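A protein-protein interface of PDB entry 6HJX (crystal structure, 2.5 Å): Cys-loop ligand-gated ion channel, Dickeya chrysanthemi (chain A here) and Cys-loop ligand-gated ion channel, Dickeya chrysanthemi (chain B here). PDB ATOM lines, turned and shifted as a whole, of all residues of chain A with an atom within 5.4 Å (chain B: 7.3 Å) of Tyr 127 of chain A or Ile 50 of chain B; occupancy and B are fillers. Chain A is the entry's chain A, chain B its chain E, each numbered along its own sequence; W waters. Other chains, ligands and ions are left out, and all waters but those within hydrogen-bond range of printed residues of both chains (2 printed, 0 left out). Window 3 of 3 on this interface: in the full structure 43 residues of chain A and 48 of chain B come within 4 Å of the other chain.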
ATOM      1  N   TRP A  64      32.565 -12.625 -30.436  1.00  0.00           N
ATOM      2  CA  TRP A  64      31.370 -12.099 -29.783  1.00  0.00           C
ATOM      3  C   TRP A  64      31.131 -12.882 -28.496  1.00  0.00           C
ATOM      4  O   TRP A  64      30.822 -14.078 -28.540  1.00  0.00           O
ATOM      5  CB  TRP A  64      30.167 -12.199 -30.719  1.00  0.00           C
ATOM      6  CG  TRP A  64      28.911 -11.596 -30.175  1.00  0.00           C
ATOM      7  CD1 TRP A  64      28.670 -10.274 -29.950  1.00  0.00           C
ATOM      8  CD2 TRP A  64      27.709 -12.289 -29.811  1.00  0.00           C
ATOM      9  NE1 TRP A  64      27.398 -10.099 -29.461  1.00  0.00           N
ATOM     10  CE2 TRP A  64      26.788 -11.323 -29.367  1.00  0.00           C
ATOM     11  CE3 TRP A  64      27.326 -13.633 -29.815  1.00  0.00           C
ATOM     12  CZ2 TRP A  64      25.508 -11.658 -28.929  1.00  0.00           C
ATOM     13  CZ3 TRP A  64      26.055 -13.964 -29.379  1.00  0.00           C
ATOM     14  CH2 TRP A  64      25.162 -12.981 -28.944  1.00  0.00           C
ATOM     15  N   PRO A  66      28.771 -12.141 -25.346  1.00  0.00           N
ATOM     16  CA  PRO A  66      27.826 -11.200 -24.732  1.00  0.00           C
ATOM     17  C   PRO A  66      27.841 -11.268 -23.211  1.00  0.00           C
ATOM     18  O   PRO A  66      27.997 -12.336 -22.615  1.00  0.00           O
ATOM     19  CB  PRO A  66      26.472 -11.646 -25.296  1.00  0.00           C
ATOM     20  CG  PRO A  66      26.642 -13.107 -25.542  1.00  0.00           C
ATOM     21  CD  PRO A  66      28.085 -13.295 -25.955  1.00  0.00           C
ATOM     22  N   ALA A  67      27.662 -10.110 -22.586  1.00  0.00           N
ATOM     23  CA  ALA A  67      27.651 -10.023 -21.132  1.00  0.00           C
ATOM     24  C   ALA A  67      26.296 -10.477 -20.599  1.00  0.00           C
ATOM     25  O   ALA A  67      25.259  -9.912 -20.963  1.00  0.00           O
ATOM     26  CB  ALA A  67      27.951  -8.594 -20.681  1.00  0.00           C
ATOM     27  N   PRO A 124      20.500 -11.156 -20.426  1.00  0.00           N
ATOM     28  CA  PRO A 124      21.525 -10.427 -21.186  1.00  0.00           C
ATOM     29  C   PRO A 124      21.495  -8.944 -20.845  1.00  0.00           C
ATOM     30  O   PRO A 124      20.434  -8.362 -20.611  1.00  0.00           O
ATOM     31  CB  PRO A 124      21.139 -10.680 -22.649  1.00  0.00           C
ATOM     32  CG  PRO A 124      20.278 -11.902 -22.616  1.00  0.00           C
ATOM     33  CD  PRO A 124      19.542 -11.835 -21.315  1.00  0.00           C
ATOM     34  N   PHE A 125      22.677  -8.330 -20.820  1.00  0.00           N
ATOM     35  CA  PHE A 125      22.763  -6.935 -20.407  1.00  0.00           C
ATOM     36  C   PHE A 125      22.418  -5.966 -21.531  1.00  0.00           C
ATOM     37  O   PHE A 125      21.955  -4.854 -21.256  1.00  0.00           O
ATOM     38  CB  PHE A 125      24.164  -6.622 -19.885  1.00  0.00           C
ATOM     39  CG  PHE A 125      24.285  -5.258 -19.283  1.00  0.00           C
ATOM     40  CD1 PHE A 125      23.851  -5.018 -17.993  1.00  0.00           C
ATOM     41  CD2 PHE A 125      24.826  -4.211 -20.008  1.00  0.00           C
ATOM     42  CE1 PHE A 125      23.954  -3.761 -17.436  1.00  0.00           C
ATOM     43  CE2 PHE A 125      24.933  -2.951 -19.455  1.00  0.00           C
ATOM     44  CZ  PHE A 125      24.498  -2.725 -18.169  1.00  0.00           C
ATOM     45  N   SER A 126      22.630  -6.356 -22.788  1.00  0.00           N
ATOM     46  CA  SER A 126      22.507  -5.427 -23.903  1.00  0.00           C
ATOM     47  C   SER A 126      21.658  -5.931 -25.060  1.00  0.00           C
ATOM     48  O   SER A 126      21.171  -5.102 -25.838  1.00  0.00           O
ATOM     49  CB  SER A 126      23.899  -5.067 -24.450  1.00  0.00           C
ATOM     50  OG  SER A 126      24.777  -4.666 -23.410  1.00  0.00           O
ATOM     51  N   TYR A 127      21.451  -7.238 -25.198  1.00  0.00           N
ATOM     52  CA  TYR A 127      20.799  -7.815 -26.368  1.00  0.00           C
ATOM     53  C   TYR A 127      19.401  -8.304 -26.013  1.00  0.00           C
ATOM     54  O   TYR A 127      19.226  -9.055 -25.044  1.00  0.00           O
ATOM     55  CB  TYR A 127      21.641  -8.963 -26.933  1.00  0.00           C
ATOM     56  CG  TYR A 127      23.050  -8.544 -27.273  1.00  0.00           C
ATOM     57  CD1 TYR A 127      23.326  -7.856 -28.450  1.00  0.00           C
ATOM     58  CD2 TYR A 127      24.106  -8.826 -26.417  1.00  0.00           C
ATOM     59  CE1 TYR A 127      24.615  -7.465 -28.765  1.00  0.00           C
ATOM     60  CE2 TYR A 127      25.397  -8.439 -26.721  1.00  0.00           C
ATOM     61  CZ  TYR A 127      25.646  -7.758 -27.896  1.00  0.00           C
ATOM     62  OH  TYR A 127      26.929  -7.372 -28.208  1.00  0.00           O
ATOM     63  N   ASN A 128      18.412  -7.884 -26.802  1.00  0.00           N
ATOM     64  CA  ASN A 128      17.032  -8.288 -26.584  1.00  0.00           C
ATOM     65  C   ASN A 128      16.806  -9.698 -27.132  1.00  0.00           C
ATOM     66  O   ASN A 128      17.704 -10.323 -27.705  1.00  0.00           O
ATOM     67  CB  ASN A 128      16.075  -7.274 -27.216  1.00  0.00           C
ATOM     68  CG  ASN A 128      16.224  -7.178 -28.727  1.00  0.00           C
ATOM     69  OD1 ASN A 128      16.502  -8.166 -29.407  1.00  0.00           O
ATOM     70  ND2 ASN A 128      16.035  -5.978 -29.258  1.00  0.00           N
ATOM     71  N   ASN A 129      15.583 -10.205 -26.955  1.00  0.00           N
ATOM     72  CA  ASN A 129      15.259 -11.576 -27.333  1.00  0.00           C
ATOM     73  C   ASN A 129      15.101 -11.762 -28.838  1.00  0.00           C
ATOM     74  O   ASN A 129      14.892 -12.896 -29.284  1.00  0.00           O
ATOM     75  CB  ASN A 129      13.985 -12.038 -26.619  1.00  0.00           C
ATOM     76  CG  ASN A 129      12.779 -11.192 -26.960  1.00  0.00           C
ATOM     77  OD1 ASN A 129      12.832 -10.332 -27.837  1.00  0.00           O
ATOM     78  ND2 ASN A 129      11.675 -11.438 -26.266  1.00  0.00           N
ATOM     79  N   GLN A 131      17.726 -10.767 -30.611  1.00  0.00           N
ATOM     80  CA  GLN A 131      19.152 -10.982 -30.832  1.00  0.00           C
ATOM     81  C   GLN A 131      19.714 -12.139 -30.014  1.00  0.00           C
ATOM     82  O   GLN A 131      20.538 -12.907 -30.524  1.00  0.00           O
ATOM     83  CB  GLN A 131      19.924  -9.705 -30.486  1.00  0.00           C
ATOM     84  CG  GLN A 131      19.544  -8.512 -31.332  1.00  0.00           C
ATOM     85  CD  GLN A 131      19.945  -7.196 -30.701  1.00  0.00           C
ATOM     86  OE1 GLN A 131      19.981  -7.062 -29.477  1.00  0.00           O
ATOM     87  NE2 GLN A 131      20.246  -6.212 -31.537  1.00  0.00           N
ATOM     88  N   LEU A 132      19.295 -12.272 -28.755  1.00  0.00           N
ATOM     89  CA  LEU A 132      19.798 -13.309 -27.858  1.00  0.00           C
ATOM     90  C   LEU A 132      18.647 -13.820 -27.006  1.00  0.00           C
ATOM     91  O   LEU A 132      18.025 -13.044 -26.273  1.00  0.00           O
ATOM     92  CB  LEU A 132      20.922 -12.767 -26.967  1.00  0.00           C
ATOM     93  CG  LEU A 132      21.859 -13.770 -26.288  1.00  0.00           C
ATOM     94  CD1 LEU A 132      23.038 -13.030 -25.685  1.00  0.00           C
ATOM     95  CD2 LEU A 132      21.153 -14.589 -25.216  1.00  0.00           C
ATOM     96  N   PHE A 180      13.436  -8.629 -23.239  1.00  0.00           N
ATOM     97  CA  PHE A 180      14.658  -9.365 -22.942  1.00  0.00           C
ATOM     98  C   PHE A 180      14.327 -10.748 -22.401  1.00  0.00           C
ATOM     99  O   PHE A 180      13.326 -10.938 -21.705  1.00  0.00           O
ATOM    100  CB  PHE A 180      15.524  -8.602 -21.935  1.00  0.00           C
ATOM    101  CG  PHE A 180      16.278  -7.455 -22.541  1.00  0.00           C
ATOM    102  CD1 PHE A 180      15.622  -6.290 -22.895  1.00  0.00           C
ATOM    103  CD2 PHE A 180      17.641  -7.545 -22.762  1.00  0.00           C
ATOM    104  CE1 PHE A 180      16.310  -5.236 -23.455  1.00  0.00           C
ATOM    105  CE2 PHE A 180      18.336  -6.495 -23.321  1.00  0.00           C
ATOM    106  CZ  PHE A 180      17.670  -5.339 -23.670  1.00  0.00           C
ATOM    107  N   SER A 181      15.184 -11.714 -22.733  1.00  0.00           N
ATOM    108  CA  SER A 181      15.030 -13.093 -22.287  1.00  0.00           C
ATOM    109  C   SER A 181      15.680 -13.264 -20.920  1.00  0.00           C
ATOM    110  O   SER A 181      16.850 -12.912 -20.738  1.00  0.00           O
ATOM    111  CB  SER A 181      15.664 -14.048 -23.303  1.00  0.00           C
ATOM    112  OG  SER A 181      15.406 -15.406 -22.989  1.00  0.00           O
ATOM    113  N   LYS B  47      22.646  -0.829 -38.352  1.00  0.00           N
ATOM    114  CA  LYS B  47      21.898  -1.074 -37.133  1.00  0.00           C
ATOM    115  C   LYS B  47      22.686  -0.576 -35.931  1.00  0.00           C
ATOM    116  O   LYS B  47      23.911  -0.434 -35.995  1.00  0.00           O
ATOM    117  CB  LYS B  47      21.602  -2.568 -36.980  1.00  0.00           C
ATOM    118  N   PRO B  48      22.019  -0.293 -34.814  1.00  0.00           N
ATOM    119  CA  PRO B  48      22.742   0.210 -33.640  1.00  0.00           C
ATOM    120  C   PRO B  48      23.860  -0.738 -33.235  1.00  0.00           C
ATOM    121  O   PRO B  48      23.714  -1.961 -33.292  1.00  0.00           O
ATOM    122  CB  PRO B  48      21.656   0.304 -32.562  1.00  0.00           C
ATOM    123  CG  PRO B  48      20.373   0.405 -33.321  1.00  0.00           C
ATOM    124  CD  PRO B  48      20.570  -0.407 -34.565  1.00  0.00           C
ATOM    125  N   LEU B  49      24.989  -0.163 -32.836  1.00  0.00           N
ATOM    126  CA  LEU B  49      26.157  -0.937 -32.437  1.00  0.00           C
ATOM    127  C   LEU B  49      26.275  -0.958 -30.918  1.00  0.00           C
ATOM    128  O   LEU B  49      25.977   0.034 -30.247  1.00  0.00           O
ATOM    129  CB  LEU B  49      27.429  -0.361 -33.055  1.00  0.00           C
ATOM    130  CG  LEU B  49      28.699  -1.176 -32.814  1.00  0.00           C
ATOM    131  CD1 LEU B  49      28.590  -2.563 -33.434  1.00  0.00           C
ATOM    132  CD2 LEU B  49      29.908  -0.441 -33.363  1.00  0.00           C
ATOM    133  N   ILE B  50      26.722  -2.093 -30.385  1.00  0.00           N
ATOM    134  CA  ILE B  50      26.782  -2.327 -28.947  1.00  0.00           C
ATOM    135  C   ILE B  50      28.231  -2.567 -28.549  1.00  0.00           C
ATOM    136  O   ILE B  50      28.911  -3.417 -29.137  1.00  0.00           O
ATOM    137  CB  ILE B  50      25.885  -3.511 -28.538  1.00  0.00           C
ATOM    138  CG1 ILE B  50      24.422  -3.054 -28.501  1.00  0.00           C
ATOM    139  CG2 ILE B  50      26.310  -4.086 -27.187  1.00  0.00           C
ATOM    140  CD1 ILE B  50      23.418  -4.180 -28.358  1.00  0.00           C
ATOM    141  N   VAL B  51      28.694  -1.820 -27.548  1.00  0.00           N
ATOM    142  CA  VAL B  51      30.042  -1.939 -27.004  1.00  0.00           C
ATOM    143  C   VAL B  51      29.922  -2.137 -25.499  1.00  0.00           C
ATOM    144  O   VAL B  51      29.270  -1.338 -24.816  1.00  0.00           O
ATOM    145  CB  VAL B  51      30.895  -0.693 -27.317  1.00  0.00           C
ATOM    146  CG1 VAL B  51      32.306  -0.846 -26.761  1.00  0.00           C
ATOM    147  CG2 VAL B  51      30.931  -0.436 -28.817  1.00  0.00           C
ATOM    148  N   GLU B  52      30.559  -3.187 -24.983  1.00  0.00           N
ATOM    149  CA  GLU B  52      30.393  -3.598 -23.594  1.00  0.00           C
ATOM    150  C   GLU B  52      31.723  -3.593 -22.857  1.00  0.00           C
ATOM    151  O   GLU B  52      32.730  -4.097 -23.370  1.00  0.00           O
ATOM    152  CB  GLU B  52      29.779  -4.998 -23.510  1.00  0.00           C
ATOM    153  CG  GLU B  52      28.307  -5.055 -23.855  1.00  0.00           C
ATOM    154  CD  GLU B  52      27.746  -6.458 -23.764  1.00  0.00           C
ATOM    155  OE1 GLU B  52      28.498  -7.421 -24.031  1.00  0.00           O
ATOM    156  OE2 GLU B  52      26.553  -6.597 -23.418  1.00  0.00           O
ATOM    157  N   GLN B  55      35.679  -3.218 -23.822  1.00  0.00           N
ATOM    158  CA  GLN B  55      35.715  -2.754 -25.204  1.00  0.00           C
ATOM    159  C   GLN B  55      35.442  -1.259 -25.307  1.00  0.00           C
ATOM    160  O   GLN B  55      35.884  -0.620 -26.268  1.00  0.00           O
ATOM    161  CB  GLN B  55      34.703  -3.530 -26.047  1.00  0.00           C
ATOM    162  CG  GLN B  55      35.079  -4.982 -26.277  1.00  0.00           C
ATOM    163  CD  GLN B  55      36.351  -5.126 -27.084  1.00  0.00           C
ATOM    164  OE1 GLN B  55      36.394  -4.770 -28.262  1.00  0.00           O
ATOM    165  NE2 GLN B  55      37.399  -5.641 -26.453  1.00  0.00           N
ATOM    166  N   ILE B  56      34.720  -0.688 -24.340  1.00  0.00           N
ATOM    167  CA  ILE B  56      34.432   0.743 -24.380  1.00  0.00           C
ATOM    168  C   ILE B  56      35.725   1.544 -24.418  1.00  0.00           C
ATOM    169  O   ILE B  56      35.804   2.596 -25.066  1.00  0.00           O
ATOM    170  CB  ILE B  56      33.556   1.148 -23.179  1.00  0.00           C
ATOM    171  CG1 ILE B  56      32.177   0.501 -23.296  1.00  0.00           C
ATOM    172  CG2 ILE B  56      33.429   2.664 -23.101  1.00  0.00           C
ATOM    173  CD1 ILE B  56      31.307   0.689 -22.076  1.00  0.00           C
ATOM    174  N   TRP B  59      37.166   2.326 -27.818  1.00  0.00           N
ATOM    175  CA  TRP B  59      36.448   3.343 -28.580  1.00  0.00           C
ATOM    176  C   TRP B  59      36.803   4.748 -28.114  1.00  0.00           C
ATOM    177  O   TRP B  59      36.938   5.660 -28.938  1.00  0.00           O
ATOM    178  CB  TRP B  59      34.945   3.100 -28.473  1.00  0.00           C
ATOM    179  CG  TRP B  59      34.525   1.902 -29.253  1.00  0.00           C
ATOM    180  CD1 TRP B  59      34.678   0.595 -28.896  1.00  0.00           C
ATOM    181  CD2 TRP B  59      33.903   1.897 -30.536  1.00  0.00           C
ATOM    182  NE1 TRP B  59      34.184  -0.225 -29.877  1.00  0.00           N
ATOM    183  CE2 TRP B  59      33.701   0.551 -30.897  1.00  0.00           C
ATOM    184  CE3 TRP B  59      33.495   2.900 -31.417  1.00  0.00           C
ATOM    185  CZ2 TRP B  59      33.107   0.184 -32.097  1.00  0.00           C
ATOM    186  CZ3 TRP B  59      32.906   2.535 -32.607  1.00  0.00           C
ATOM    187  CH2 TRP B  59      32.717   1.189 -32.937  1.00  0.00           C
ATOM    188  N   ARG B  84      27.647  -0.281 -20.872  1.00  0.00           N
ATOM    189  CA  ARG B  84      27.347  -0.495 -22.279  1.00  0.00           C
ATOM    190  C   ARG B  84      27.208   0.836 -22.999  1.00  0.00           C
ATOM    191  O   ARG B  84      26.636   1.788 -22.461  1.00  0.00           O
ATOM    192  CB  ARG B  84      26.054  -1.308 -22.425  1.00  0.00           C
ATOM    193  CG  ARG B  84      25.637  -1.611 -23.848  1.00  0.00           C
ATOM    194  CD  ARG B  84      24.121  -1.622 -23.953  1.00  0.00           C
ATOM    195  NE  ARG B  84      23.574  -0.267 -23.944  1.00  0.00           N
ATOM    196  CZ  ARG B  84      22.312   0.034 -23.656  1.00  0.00           C
ATOM    197  NH1 ARG B  84      21.448  -0.920 -23.332  1.00  0.00           N
ATOM    198  NH2 ARG B  84      21.915   1.299 -23.680  1.00  0.00           N
ATOM    199  N   LEU B  85      27.734   0.889 -24.220  1.00  0.00           N
ATOM    200  CA  LEU B  85      27.465   1.968 -25.159  1.00  0.00           C
ATOM    201  C   LEU B  85      26.629   1.435 -26.316  1.00  0.00           C
ATOM    202  O   LEU B  85      26.892   0.345 -26.834  1.00  0.00           O
ATOM    203  CB  LEU B  85      28.761   2.570 -25.709  1.00  0.00           C
ATOM    204  CG  LEU B  85      29.599   3.443 -24.778  1.00  0.00           C
ATOM    205  CD1 LEU B  85      30.918   3.759 -25.451  1.00  0.00           C
ATOM    206  CD2 LEU B  85      28.867   4.726 -24.413  1.00  0.00           C
ATOM    207  N   MET B  86      25.622   2.206 -26.717  1.00  0.00           N
ATOM    208  CA  MET B  86      24.844   1.917 -27.919  1.00  0.00           C
ATOM    209  C   MET B  86      25.012   3.090 -28.876  1.00  0.00           C
ATOM    210  O   MET B  86      24.574   4.206 -28.577  1.00  0.00           O
ATOM    211  CB  MET B  86      23.370   1.684 -27.591  1.00  0.00           C
ATOM    212  CG  MET B  86      22.562   1.134 -28.764  1.00  0.00           C
ATOM    213  SD  MET B  86      20.926   0.511 -28.317  1.00  0.00           S
ATOM    214  CE  MET B  86      21.358  -0.880 -27.269  1.00  0.00           C
ATOM    215  N   LEU B  87      25.647   2.837 -30.018  1.00  0.00           N
ATOM    216  CA  LEU B  87      25.942   3.870 -31.003  1.00  0.00           C
ATOM    217  C   LEU B  87      25.018   3.695 -32.201  1.00  0.00           C
ATOM    218  O   LEU B  87      24.988   2.622 -32.815  1.00  0.00           O
ATOM    219  CB  LEU B  87      27.405   3.808 -31.441  1.00  0.00           C
ATOM    220  CG  LEU B  87      28.438   3.782 -30.310  1.00  0.00           C
ATOM    221  CD1 LEU B  87      29.851   3.777 -30.875  1.00  0.00           C
ATOM    222  CD2 LEU B  87      28.245   4.956 -29.365  1.00  0.00           C
HETATM  223  O   HOH W   1      24.707  -8.308 -23.220  1.00  0.00           O
HETATM  224  O   HOH W   2      28.995  -7.681 -26.706  1.00  0.00           O
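The backbone carbonyl oxygen of Ala 67 of chain A lies within hydrogen-bond range of the backbone NH of Phe 125 of chain A, at 3.0 Å.
NE1 of Trp 64 of chain A is in hydrogen-bond range of OH of Tyr 127 of chain A (3.0 Å).
OG of Ser 126 of chain A sits at hydrogen-bond distance from OE2 of Glu 52 of chain B (2.6 Å).
The backbone NH (N) of Ala 67 of chain A lies within hydrogen-bond range of the side-chain carboxylate (OE1) of Glu 52 of chain B, at 3.2 Å.
Water W1 lies within hydrogen-bond range of OE2 of Glu 52 of chain B, O of Ala 67 of chain A, N of Ser 126 of chain A and N of Phe 125 of chain A.
Water W2 bridges the side-chain hydroxyl (OH) of Tyr 127 of chain A (2.6 Å) and the side-chain carboxylate (OE1) of Glu 52 of chain B (2.7 Å).
Of the printed residues of chain B, Ala 67 of chain A touches Glu 52.
Of the printed residues of chain B, Ser 126 of chain A touches Ile 50 (3.5 Å), Glu 52 (2.6 Å) and Arg 84 (3.2 Å).
Tyr 127 of chain A touches two residues of chain B.
Of chain A, only Ser 126 (3.5 Å) and Tyr 127 (3.5 Å) come within 4 Å of Ile 50 of chain B.
Printed residues of chain A within 4 Å of Glu 52 of chain B: Pro 66 (3.9 Å), Ala 67 (3.2 Å), Ser 126 (2.6 Å) and Tyr 127 (3.95 Å).
The nearest printed residue of chain B that does not touch Pro 66 of chain A is Ile 50 of chain B (7.7 Å).
Of the 13 printed residues of chain A, 5 touch a printed residue of chain B.
Hydrophobic or aromatic side chains of chain A within 4 Å of the printed part of chain B: Ala 67, Phe 125 and Tyr 127.
Printed residues of chain B that touch a printed residue of chain A: Ile 50, Glu 52 and Arg 84.
Hydrophobic or aromatic side chains of chain B within 4 Å of the printed part of chain A: Ile 50.
Along chain B the printed residues that touch a printed residue of chain A span positions 50 to 84.
Among the printed residues, 8 pairs touch across the chains.
Among the printed residues, no Asp or Glu carboxylate lies within 4 Å of a Lys or Arg side-chain nitrogen of the other chain.
Among the printed residues, merely in contact across the chains: Pro 66 of chain A with Glu 52 of chain B, Phe 125 of chain A with Arg 84 of chain B, Ser 126 of chain A with Ile 50 of chain B, Ser 126 of chain A with Arg 84 of chain B, Tyr 127 of chain A with Ile 50 of chain B and Tyr 127 of chain A with Glu 52 of chain B.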
